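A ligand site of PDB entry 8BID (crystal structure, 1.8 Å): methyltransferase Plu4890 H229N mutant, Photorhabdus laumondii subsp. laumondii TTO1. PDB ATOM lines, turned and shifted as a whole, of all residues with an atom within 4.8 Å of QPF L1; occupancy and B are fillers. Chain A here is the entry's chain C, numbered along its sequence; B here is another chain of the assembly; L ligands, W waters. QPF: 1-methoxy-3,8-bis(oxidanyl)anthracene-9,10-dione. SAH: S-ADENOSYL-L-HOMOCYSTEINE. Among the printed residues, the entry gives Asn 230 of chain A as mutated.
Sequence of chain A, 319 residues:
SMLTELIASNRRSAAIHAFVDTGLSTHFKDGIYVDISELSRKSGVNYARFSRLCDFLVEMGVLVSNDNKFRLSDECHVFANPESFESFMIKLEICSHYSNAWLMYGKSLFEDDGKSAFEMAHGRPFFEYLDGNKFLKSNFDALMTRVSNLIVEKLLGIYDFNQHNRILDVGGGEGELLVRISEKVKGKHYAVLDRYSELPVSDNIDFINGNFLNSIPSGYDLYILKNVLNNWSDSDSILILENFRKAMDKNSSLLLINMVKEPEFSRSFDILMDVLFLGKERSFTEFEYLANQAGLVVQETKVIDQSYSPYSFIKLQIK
The side-chain amide nitrogen (ND2) of Asn 230 sits at hydrogen-bond distance from an oxygen (OAI) of QPF L1. OAI of QPF L1 sits at hydrogen-bond distance from O of Asn 227, at 2.9 Å. The side-chain amide oxygen (OD1) of Asn 231 lies within hydrogen-bond range of an oxygen (OAI) of QPF L1 (3.0 Å).
The side-chain amide oxygen (OD1) of Asn 230 lies close to the backbone carbonyl oxygen (O) of Asn 227. The side-chain sulfur of Met 273 sits at hydrogen-bond distance from the side-chain amide nitrogen of Asn 230, 3.7 Å away. The side-chain amide oxygen (OD1) of Asn 227 is in hydrogen-bond range of the backbone NH (N) of Met 259 (3.3 Å). OH of Tyr 311 lies within hydrogen-bond range of ND2 of Asn 227 (3.0 Å). The side-chain hydroxyl (OH) of Tyr 308 is in hydrogen-bond range of the side-chain hydroxyl (OH) of Tyr 311, 3.3 Å away.
Met 89 touches QPF L1 (CG to OAS, 3.6 Å). Phe 140 touches QPF L1 (CE1 to CAM, 3.4 Å). Leu 143 touches QPF L1. CE of Met 144 touches CAF of QPF L1 (3.5 Å). CE of Met 259 touches OAE of QPF L1 (3.7 Å). Phe 269 touches QPF L1 (CE1 to CAN, 3.6 Å). Met 273 touches QPF L1 (CE to OAL, 3.8 Å). Leu 276 touches QPF L1 (CD1 to CAM, 3.5 Å). Phe 277 touches QPF L1 (CE2 to CAM, 3.9 Å). CE1 of Tyr 308 touches CAA of QPF L1, 3.9 Å away. Tyr 311 touches QPF L1 (OH to OAE, 3.9 Å). Hydrophobic or aromatic side chains that line QPF L1: Met 89, Phe 140, Leu 143, Met 144, Met 259, Phe 269, Met 273, Leu 276, Phe 277 and Tyr 308. 14 residues have an atom within 4 Å of QPF L1: Met 89, Phe 140, Leu 143, Met 144, Asn 227, Asn 230, Asn 231, Met 259, Phe 269, Met 273, Leu 276, Phe 277, Tyr 308 and Tyr 311. The nearest printed residue that does not touch QPF L1 is Val 147 (4.01 Å).
Water W1 lies within hydrogen-bond range of OH of Tyr 98 (2.8 Å) and OAP of QPF L1 (3.4 Å).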
ATOM      1  N   PHE A  85     -19.813  -3.005  34.726  1.00  0.00           N
ATOM      2  CA  PHE A  85     -19.061  -2.452  33.561  1.00  0.00           C
ATOM      3  C   PHE A  85     -18.771  -3.576  32.567  1.00  0.00           C
ATOM      4  O   PHE A  85     -18.816  -3.318  31.349  1.00  0.00           O
ATOM      5  CB  PHE A  85     -17.829  -1.659  33.990  1.00  0.00           C
ATOM      6  CG  PHE A  85     -16.533  -2.417  34.115  1.00  0.00           C
ATOM      7  CD1 PHE A  85     -15.788  -2.746  32.995  1.00  0.00           C
ATOM      8  CD2 PHE A  85     -16.028  -2.762  35.369  1.00  0.00           C
ATOM      9  CE1 PHE A  85     -14.587  -3.415  33.121  1.00  0.00           C
ATOM     10  CE2 PHE A  85     -14.822  -3.438  35.485  1.00  0.00           C
ATOM     11  CZ  PHE A  85     -14.106  -3.769  34.362  1.00  0.00           C
ATOM     12  N   MET A  89     -19.180  -3.743  28.588  1.00  0.00           N
ATOM     13  CA  MET A  89     -17.918  -3.938  27.812  1.00  0.00           C
ATOM     14  C   MET A  89     -18.131  -4.992  26.717  1.00  0.00           C
ATOM     15  O   MET A  89     -17.759  -4.732  25.564  1.00  0.00           O
ATOM     16  CB  MET A  89     -16.772  -4.377  28.718  1.00  0.00           C
ATOM     17  CG  MET A  89     -15.419  -4.410  28.008  1.00  0.00           C
ATOM     18  SD  MET A  89     -14.109  -5.157  29.009  1.00  0.00           S
ATOM     19  CE  MET A  89     -12.737  -5.127  27.842  1.00  0.00           C
ATOM     20  N   TYR A  98     -17.979  -2.122  15.938  1.00  0.00           N
ATOM     21  CA  TYR A  98     -16.590  -2.410  16.392  1.00  0.00           C
ATOM     22  C   TYR A  98     -15.959  -3.414  15.416  1.00  0.00           C
ATOM     23  O   TYR A  98     -14.824  -3.169  14.935  1.00  0.00           O
ATOM     24  CB  TYR A  98     -16.558  -2.886  17.854  1.00  0.00           C
ATOM     25  CG  TYR A  98     -16.648  -1.821  18.920  1.00  0.00           C
ATOM     26  CD1 TYR A  98     -15.822  -1.860  20.040  1.00  0.00           C
ATOM     27  CD2 TYR A  98     -17.583  -0.800  18.861  1.00  0.00           C
ATOM     28  CE1 TYR A  98     -15.907  -0.917  21.046  1.00  0.00           C
ATOM     29  CE2 TYR A  98     -17.685   0.160  19.865  1.00  0.00           C
ATOM     30  CZ  TYR A  98     -16.842   0.107  20.957  1.00  0.00           C
ATOM     31  OH  TYR A  98     -16.942   1.050  21.947  1.00  0.00           O
ATOM     32  N   PHE A 140     -21.940   3.000  25.518  1.00  0.00           N
ATOM     33  CA  PHE A 140     -20.596   3.590  25.737  1.00  0.00           C
ATOM     34  C   PHE A 140     -20.635   4.503  26.964  1.00  0.00           C
ATOM     35  O   PHE A 140     -19.734   4.395  27.843  1.00  0.00           O
ATOM     36  CB  PHE A 140     -20.092   4.337  24.500  1.00  0.00           C
ATOM     37  CG  PHE A 140     -18.737   4.946  24.720  1.00  0.00           C
ATOM     38  CD1 PHE A 140     -17.589   4.190  24.567  1.00  0.00           C
ATOM     39  CD2 PHE A 140     -18.605   6.265  25.137  1.00  0.00           C
ATOM     40  CE1 PHE A 140     -16.339   4.747  24.811  1.00  0.00           C
ATOM     41  CE2 PHE A 140     -17.356   6.824  25.352  1.00  0.00           C
ATOM     42  CZ  PHE A 140     -16.231   6.055  25.215  1.00  0.00           C
ATOM     43  N   LEU A 143     -20.913   2.345  30.122  1.00  0.00           N
ATOM     44  CA  LEU A 143     -19.599   1.751  30.472  1.00  0.00           C
ATOM     45  C   LEU A 143     -18.770   2.794  31.223  1.00  0.00           C
ATOM     46  O   LEU A 143     -18.227   2.453  32.296  1.00  0.00           O
ATOM     47  CB  LEU A 143     -18.887   1.273  29.202  1.00  0.00           C
ATOM     48  CG  LEU A 143     -17.442   0.801  29.404  1.00  0.00           C
ATOM     49  CD1 LEU A 143     -17.378  -0.446  30.261  1.00  0.00           C
ATOM     50  CD2 LEU A 143     -16.779   0.558  28.062  1.00  0.00           C
ATOM     51  N   MET A 144     -18.688   4.017  30.695  1.00  0.00           N
ATOM     52  CA  MET A 144     -17.849   5.101  31.271  1.00  0.00           C
ATOM     53  C   MET A 144     -18.395   5.459  32.669  1.00  0.00           C
ATOM     54  O   MET A 144     -17.599   5.670  33.594  1.00  0.00           O
ATOM     55  CB  MET A 144     -17.832   6.353  30.382  1.00  0.00           C
ATOM     56  CG  MET A 144     -17.168   6.152  29.020  1.00  0.00           C
ATOM     57  SD  MET A 144     -15.448   5.572  29.085  1.00  0.00           S
ATOM     58  CE  MET A 144     -15.667   3.834  28.752  1.00  0.00           C
ATOM     59  N   VAL A 147     -17.133   2.589  35.201  1.00  0.00           N
ATOM     60  CA  VAL A 147     -15.686   2.628  35.568  1.00  0.00           C
ATOM     61  C   VAL A 147     -15.403   3.904  36.377  1.00  0.00           C
ATOM     62  O   VAL A 147     -14.541   3.840  37.280  1.00  0.00           O
ATOM     63  CB  VAL A 147     -14.749   2.487  34.347  1.00  0.00           C
ATOM     64  CG1 VAL A 147     -14.968   1.153  33.656  1.00  0.00           C
ATOM     65  CG2 VAL A 147     -14.870   3.631  33.350  1.00  0.00           C
ATOM     66  N   ASN A 227      -9.839  10.091  31.180  1.00  0.00           N
ATOM     67  CA  ASN A 227     -10.006   9.115  30.060  1.00  0.00           C
ATOM     68  C   ASN A 227     -10.457   9.826  28.781  1.00  0.00           C
ATOM     69  O   ASN A 227     -11.287   9.251  28.038  1.00  0.00           O
ATOM     70  CB  ASN A 227     -10.977   7.996  30.447  1.00  0.00           C
ATOM     71  CG  ASN A 227     -10.379   7.027  31.440  1.00  0.00           C
ATOM     72  OD1 ASN A 227      -9.173   6.834  31.477  1.00  0.00           O
ATOM     73  ND2 ASN A 227     -11.234   6.407  32.232  1.00  0.00           N
ATOM     74  N   ASN A 230      -6.733   9.584  25.615  1.00  0.00           N
ATOM     75  CA  ASN A 230      -6.555   8.274  24.927  1.00  0.00           C
ATOM     76  C   ASN A 230      -7.369   8.233  23.628  1.00  0.00           C
ATOM     77  O   ASN A 230      -7.056   7.369  22.793  1.00  0.00           O
ATOM     78  CB  ASN A 230      -6.908   7.071  25.817  1.00  0.00           C
ATOM     79  CG  ASN A 230      -8.172   7.254  26.619  1.00  0.00           C
ATOM     80  OD1 ASN A 230      -8.398   8.317  27.183  1.00  0.00           O
ATOM     81  ND2 ASN A 230      -8.990   6.217  26.711  1.00  0.00           N
ATOM     82  N   ASN A 231      -8.344   9.132  23.460  1.00  0.00           N
ATOM     83  CA  ASN A 231      -9.222   9.208  22.261  1.00  0.00           C
ATOM     84  C   ASN A 231      -8.659  10.207  21.235  1.00  0.00           C
ATOM     85  O   ASN A 231      -9.380  10.452  20.249  1.00  0.00           O
ATOM     86  CB  ASN A 231     -10.645   9.623  22.605  1.00  0.00           C
ATOM     87  CG  ASN A 231     -11.229   8.911  23.806  1.00  0.00           C
ATOM     88  OD1 ASN A 231     -10.870   7.778  24.114  1.00  0.00           O
ATOM     89  ND2 ASN A 231     -12.123   9.579  24.499  1.00  0.00           N
ATOM     90  N   MET A 259      -6.212   5.655  32.301  1.00  0.00           N
ATOM     91  CA  MET A 259      -5.576   4.312  32.190  1.00  0.00           C
ATOM     92  C   MET A 259      -4.189   4.535  31.591  1.00  0.00           C
ATOM     93  O   MET A 259      -4.096   5.289  30.595  1.00  0.00           O
ATOM     94  CB  MET A 259      -6.388   3.366  31.312  1.00  0.00           C
ATOM     95  CG  MET A 259      -7.545   2.736  32.043  1.00  0.00           C
ATOM     96  SD  MET A 259      -7.993   1.134  31.354  1.00  0.00           S
ATOM     97  CE  MET A 259      -8.531   1.621  29.719  1.00  0.00           C
ATOM     98  N   PHE A 269      -5.413  -2.615  24.464  1.00  0.00           N
ATOM     99  CA  PHE A 269      -6.174  -1.351  24.619  1.00  0.00           C
ATOM    100  C   PHE A 269      -5.564  -0.289  23.700  1.00  0.00           C
ATOM    101  O   PHE A 269      -6.330   0.434  23.031  1.00  0.00           O
ATOM    102  CB  PHE A 269      -6.221  -0.883  26.071  1.00  0.00           C
ATOM    103  CG  PHE A 269      -7.156   0.279  26.303  1.00  0.00           C
ATOM    104  CD1 PHE A 269      -8.535   0.088  26.368  1.00  0.00           C
ATOM    105  CD2 PHE A 269      -6.662   1.567  26.483  1.00  0.00           C
ATOM    106  CE1 PHE A 269      -9.398   1.154  26.571  1.00  0.00           C
ATOM    107  CE2 PHE A 269      -7.526   2.634  26.686  1.00  0.00           C
ATOM    108  CZ  PHE A 269      -8.887   2.423  26.737  1.00  0.00           C
ATOM    109  N   LEU A 272      -6.923  -0.864  20.314  1.00  0.00           N
ATOM    110  CA  LEU A 272      -8.350  -0.458  20.224  1.00  0.00           C
ATOM    111  C   LEU A 272      -8.427   1.064  20.022  1.00  0.00           C
ATOM    112  O   LEU A 272      -9.275   1.513  19.230  1.00  0.00           O
ATOM    113  CB  LEU A 272      -9.119  -0.874  21.470  1.00  0.00           C
ATOM    114  CG  LEU A 272     -10.617  -0.621  21.410  1.00  0.00           C
ATOM    115  CD1 LEU A 272     -11.265  -1.488  20.338  1.00  0.00           C
ATOM    116  CD2 LEU A 272     -11.276  -0.870  22.773  1.00  0.00           C
ATOM    117  N   MET A 273      -7.609   1.842  20.743  1.00  0.00           N
ATOM    118  CA  MET A 273      -7.633   3.318  20.664  1.00  0.00           C
ATOM    119  C   MET A 273      -7.226   3.741  19.252  1.00  0.00           C
ATOM    120  O   MET A 273      -7.843   4.704  18.741  1.00  0.00           O
ATOM    121  CB  MET A 273      -6.717   3.965  21.705  1.00  0.00           C
ATOM    122  CG  MET A 273      -7.147   3.753  23.160  1.00  0.00           C
ATOM    123  SD  MET A 273      -8.850   4.268  23.561  1.00  0.00           S
ATOM    124  CE  MET A 273      -9.738   2.738  23.284  1.00  0.00           C
ATOM    125  N   LEU A 276     -10.428   2.870  16.937  1.00  0.00           N
ATOM    126  CA  LEU A 276     -11.647   3.686  17.173  1.00  0.00           C
ATOM    127  C   LEU A 276     -11.366   5.183  16.952  1.00  0.00           C
ATOM    128  O   LEU A 276     -12.315   5.863  16.507  1.00  0.00           O
ATOM    129  CB  LEU A 276     -12.180   3.441  18.584  1.00  0.00           C
ATOM    130  CG  LEU A 276     -12.685   2.031  18.859  1.00  0.00           C
ATOM    131  CD1 LEU A 276     -13.275   1.953  20.253  1.00  0.00           C
ATOM    132  CD2 LEU A 276     -13.727   1.594  17.823  1.00  0.00           C
ATOM    133  N   PHE A 277     -10.157   5.683  17.247  1.00  0.00           N
ATOM    134  CA  PHE A 277      -9.905   7.153  17.405  1.00  0.00           C
ATOM    135  C   PHE A 277      -8.645   7.661  16.690  1.00  0.00           C
ATOM    136  O   PHE A 277      -8.498   8.898  16.650  1.00  0.00           O
ATOM    137  CB  PHE A 277      -9.759   7.507  18.882  1.00  0.00           C
ATOM    138  CG  PHE A 277     -10.921   7.112  19.767  1.00  0.00           C
ATOM    139  CD1 PHE A 277     -12.146   7.737  19.652  1.00  0.00           C
ATOM    140  CD2 PHE A 277     -10.776   6.109  20.711  1.00  0.00           C
ATOM    141  CE1 PHE A 277     -13.212   7.361  20.466  1.00  0.00           C
ATOM    142  CE2 PHE A 277     -11.842   5.733  21.525  1.00  0.00           C
ATOM    143  CZ  PHE A 277     -13.052   6.361  21.396  1.00  0.00           C
ATOM    144  N   TYR A 308      -8.619  -4.163  36.831  1.00  0.00           N
ATOM    145  CA  TYR A 308      -8.358  -4.496  35.411  1.00  0.00           C
ATOM    146  C   TYR A 308      -7.069  -3.804  34.922  1.00  0.00           C
ATOM    147  O   TYR A 308      -6.403  -4.394  34.056  1.00  0.00           O
ATOM    148  CB  TYR A 308      -9.557  -4.131  34.523  1.00  0.00           C
ATOM    149  CG  TYR A 308     -10.050  -2.709  34.654  1.00  0.00           C
ATOM    150  CD1 TYR A 308      -9.579  -1.698  33.829  1.00  0.00           C
ATOM    151  CD2 TYR A 308     -11.020  -2.378  35.592  1.00  0.00           C
ATOM    152  CE1 TYR A 308     -10.043  -0.398  33.940  1.00  0.00           C
ATOM    153  CE2 TYR A 308     -11.493  -1.085  35.723  1.00  0.00           C
ATOM    154  CZ  TYR A 308     -11.010  -0.086  34.893  1.00  0.00           C
ATOM    155  OH  TYR A 308     -11.464   1.190  35.025  1.00  0.00           O
ATOM    156  N   TYR A 311      -3.983   3.140  36.707  1.00  0.00           N
ATOM    157  CA  TYR A 311      -4.365   4.504  36.296  1.00  0.00           C
ATOM    158  C   TYR A 311      -3.252   5.484  36.675  1.00  0.00           C
ATOM    159  O   TYR A 311      -2.627   5.309  37.732  1.00  0.00           O
ATOM    160  CB  TYR A 311      -5.681   4.921  36.980  1.00  0.00           C
ATOM    161  CG  TYR A 311      -6.928   4.718  36.162  1.00  0.00           C
ATOM    162  CD1 TYR A 311      -7.593   5.798  35.590  1.00  0.00           C
ATOM    163  CD2 TYR A 311      -7.480   3.459  35.999  1.00  0.00           C
ATOM    164  CE1 TYR A 311      -8.758   5.623  34.867  1.00  0.00           C
ATOM    165  CE2 TYR A 311      -8.641   3.270  35.278  1.00  0.00           C
ATOM    166  CZ  TYR A 311      -9.290   4.356  34.709  1.00  0.00           C
ATOM    167  OH  TYR A 311     -10.444   4.163  33.994  1.00  0.00           O
ATOM    168  N   ARG B  11      -9.645  -9.091  20.060  1.00  0.00           N
ATOM    169  CA  ARG B  11      -8.600  -8.117  19.654  1.00  0.00           C
ATOM    170  C   ARG B  11      -7.380  -8.872  19.105  1.00  0.00           C
ATOM    171  O   ARG B  11      -6.692  -8.329  18.224  1.00  0.00           O
ATOM    172  CB  ARG B  11      -8.235  -7.169  20.805  1.00  0.00           C
ATOM    173  CG  ARG B  11      -9.389  -6.310  21.310  1.00  0.00           C
ATOM    174  CD  ARG B  11      -8.972  -5.271  22.326  1.00  0.00           C
ATOM    175  NE  ARG B  11     -10.108  -4.825  23.149  1.00  0.00           N
ATOM    176  CZ  ARG B  11      -9.998  -4.162  24.301  1.00  0.00           C
ATOM    177  NH1 ARG B  11     -11.087  -3.832  24.977  1.00  0.00           N
ATOM    178  NH2 ARG B  11      -8.808  -3.841  24.781  1.00  0.00           N
HETATM  179  OAE QPF L   1     -11.710   3.300  30.421  1.00  0.00           O
HETATM  180  CAD QPF L   1     -12.084   2.664  29.433  1.00  0.00           C
HETATM  181  CAC QPF L   1     -12.366   1.306  29.544  1.00  0.00           C
HETATM  182  CAB QPF L   1     -12.222   0.660  30.771  1.00  0.00           C
HETATM  183  CAA QPF L   1     -12.495  -0.700  30.905  1.00  0.00           C
HETATM  184  CAT QPF L   1     -12.909  -1.426  29.814  1.00  0.00           C
HETATM  185  CAR QPF L   1     -13.055  -0.789  28.583  1.00  0.00           C
HETATM  186  OAS QPF L   1     -13.453  -1.477  27.472  1.00  0.00           O
HETATM  187  CAQ QPF L   1     -12.789   0.571  28.426  1.00  0.00           C
HETATM  188  CAO QPF L   1     -12.946   1.195  27.181  1.00  0.00           C
HETATM  189  OAP QPF L   1     -13.309   0.546  26.189  1.00  0.00           O
HETATM  190  CAN QPF L   1     -12.667   2.575  27.072  1.00  0.00           C
HETATM  191  CAF QPF L   1     -12.237   3.306  28.196  1.00  0.00           C
HETATM  192  CAG QPF L   1     -11.969   4.667  28.086  1.00  0.00           C
HETATM  193  CAH QPF L   1     -12.125   5.325  26.863  1.00  0.00           C
HETATM  194  OAI QPF L   1     -11.853   6.674  26.755  1.00  0.00           O
HETATM  195  CAJ QPF L   1     -12.539   4.601  25.743  1.00  0.00           C
HETATM  196  CAK QPF L   1     -12.815   3.235  25.843  1.00  0.00           C
HETATM  197  OAL QPF L   1     -13.231   2.427  24.810  1.00  0.00           O
HETATM  198  CAM QPF L   1     -13.662   2.993  23.570  1.00  0.00           C
HETATM  199  N   SAH L   2     -14.712  11.534  31.570  1.00  0.00           N
HETATM  200  CA  SAH L   2     -15.682  10.409  31.438  1.00  0.00           C
HETATM  201  CB  SAH L   2     -15.943  10.058  29.971  1.00  0.00           C
HETATM  202  CG  SAH L   2     -14.695   9.813  29.140  1.00  0.00           C
HETATM  203  SD  SAH L   2     -15.079   9.180  27.491  1.00  0.00           S
HETATM  204  C   SAH L   2     -15.125   9.186  32.166  1.00  0.00           C
HETATM  205  O   SAH L   2     -15.882   8.323  32.591  1.00  0.00           O
HETATM  206  OXT SAH L   2     -13.916   9.078  32.340  1.00  0.00           O
HETATM  207  C5' SAH L   2     -14.737  10.640  26.457  1.00  0.00           C
HETATM  208  C4' SAH L   2     -15.759  11.751  26.600  1.00  0.00           C
HETATM  209  O4' SAH L   2     -15.358  12.893  25.796  1.00  0.00           O
HETATM  210  C3' SAH L   2     -17.177  11.385  26.119  1.00  0.00           C
HETATM  211  O3' SAH L   2     -18.117  11.639  27.163  1.00  0.00           O
HETATM  212  C2' SAH L   2     -17.398  12.294  24.899  1.00  0.00           C
HETATM  213  O2' SAH L   2     -18.743  12.691  24.733  1.00  0.00           O
HETATM  214  C1' SAH L   2     -16.520  13.483  25.268  1.00  0.00           C
HETATM  215  N9  SAH L   2     -16.145  14.344  24.150  1.00  0.00           N
HETATM  216  C8  SAH L   2     -15.695  13.952  22.908  1.00  0.00           C
HETATM  217  N7  SAH L   2     -15.405  14.956  22.123  1.00  0.00           N
HETATM  218  C5  SAH L   2     -15.674  16.085  22.889  1.00  0.00           C
HETATM  219  C6  SAH L   2     -15.548  17.455  22.612  1.00  0.00           C
HETATM  220  N6  SAH L   2     -15.108  17.948  21.455  1.00  0.00           N
HETATM  221  N1  SAH L   2     -15.883  18.323  23.602  1.00  0.00           N
HETATM  222  C2  SAH L   2     -16.325  17.825  24.772  1.00  0.00           C
HETATM  223  N3  SAH L   2     -16.481  16.559  25.137  1.00  0.00           N
HETATM  224  C4  SAH L   2     -16.131  15.724  24.140  1.00  0.00           C
HETATM  225  O   HOH W   1     -16.007  -0.128  24.288  1.00  0.00           O
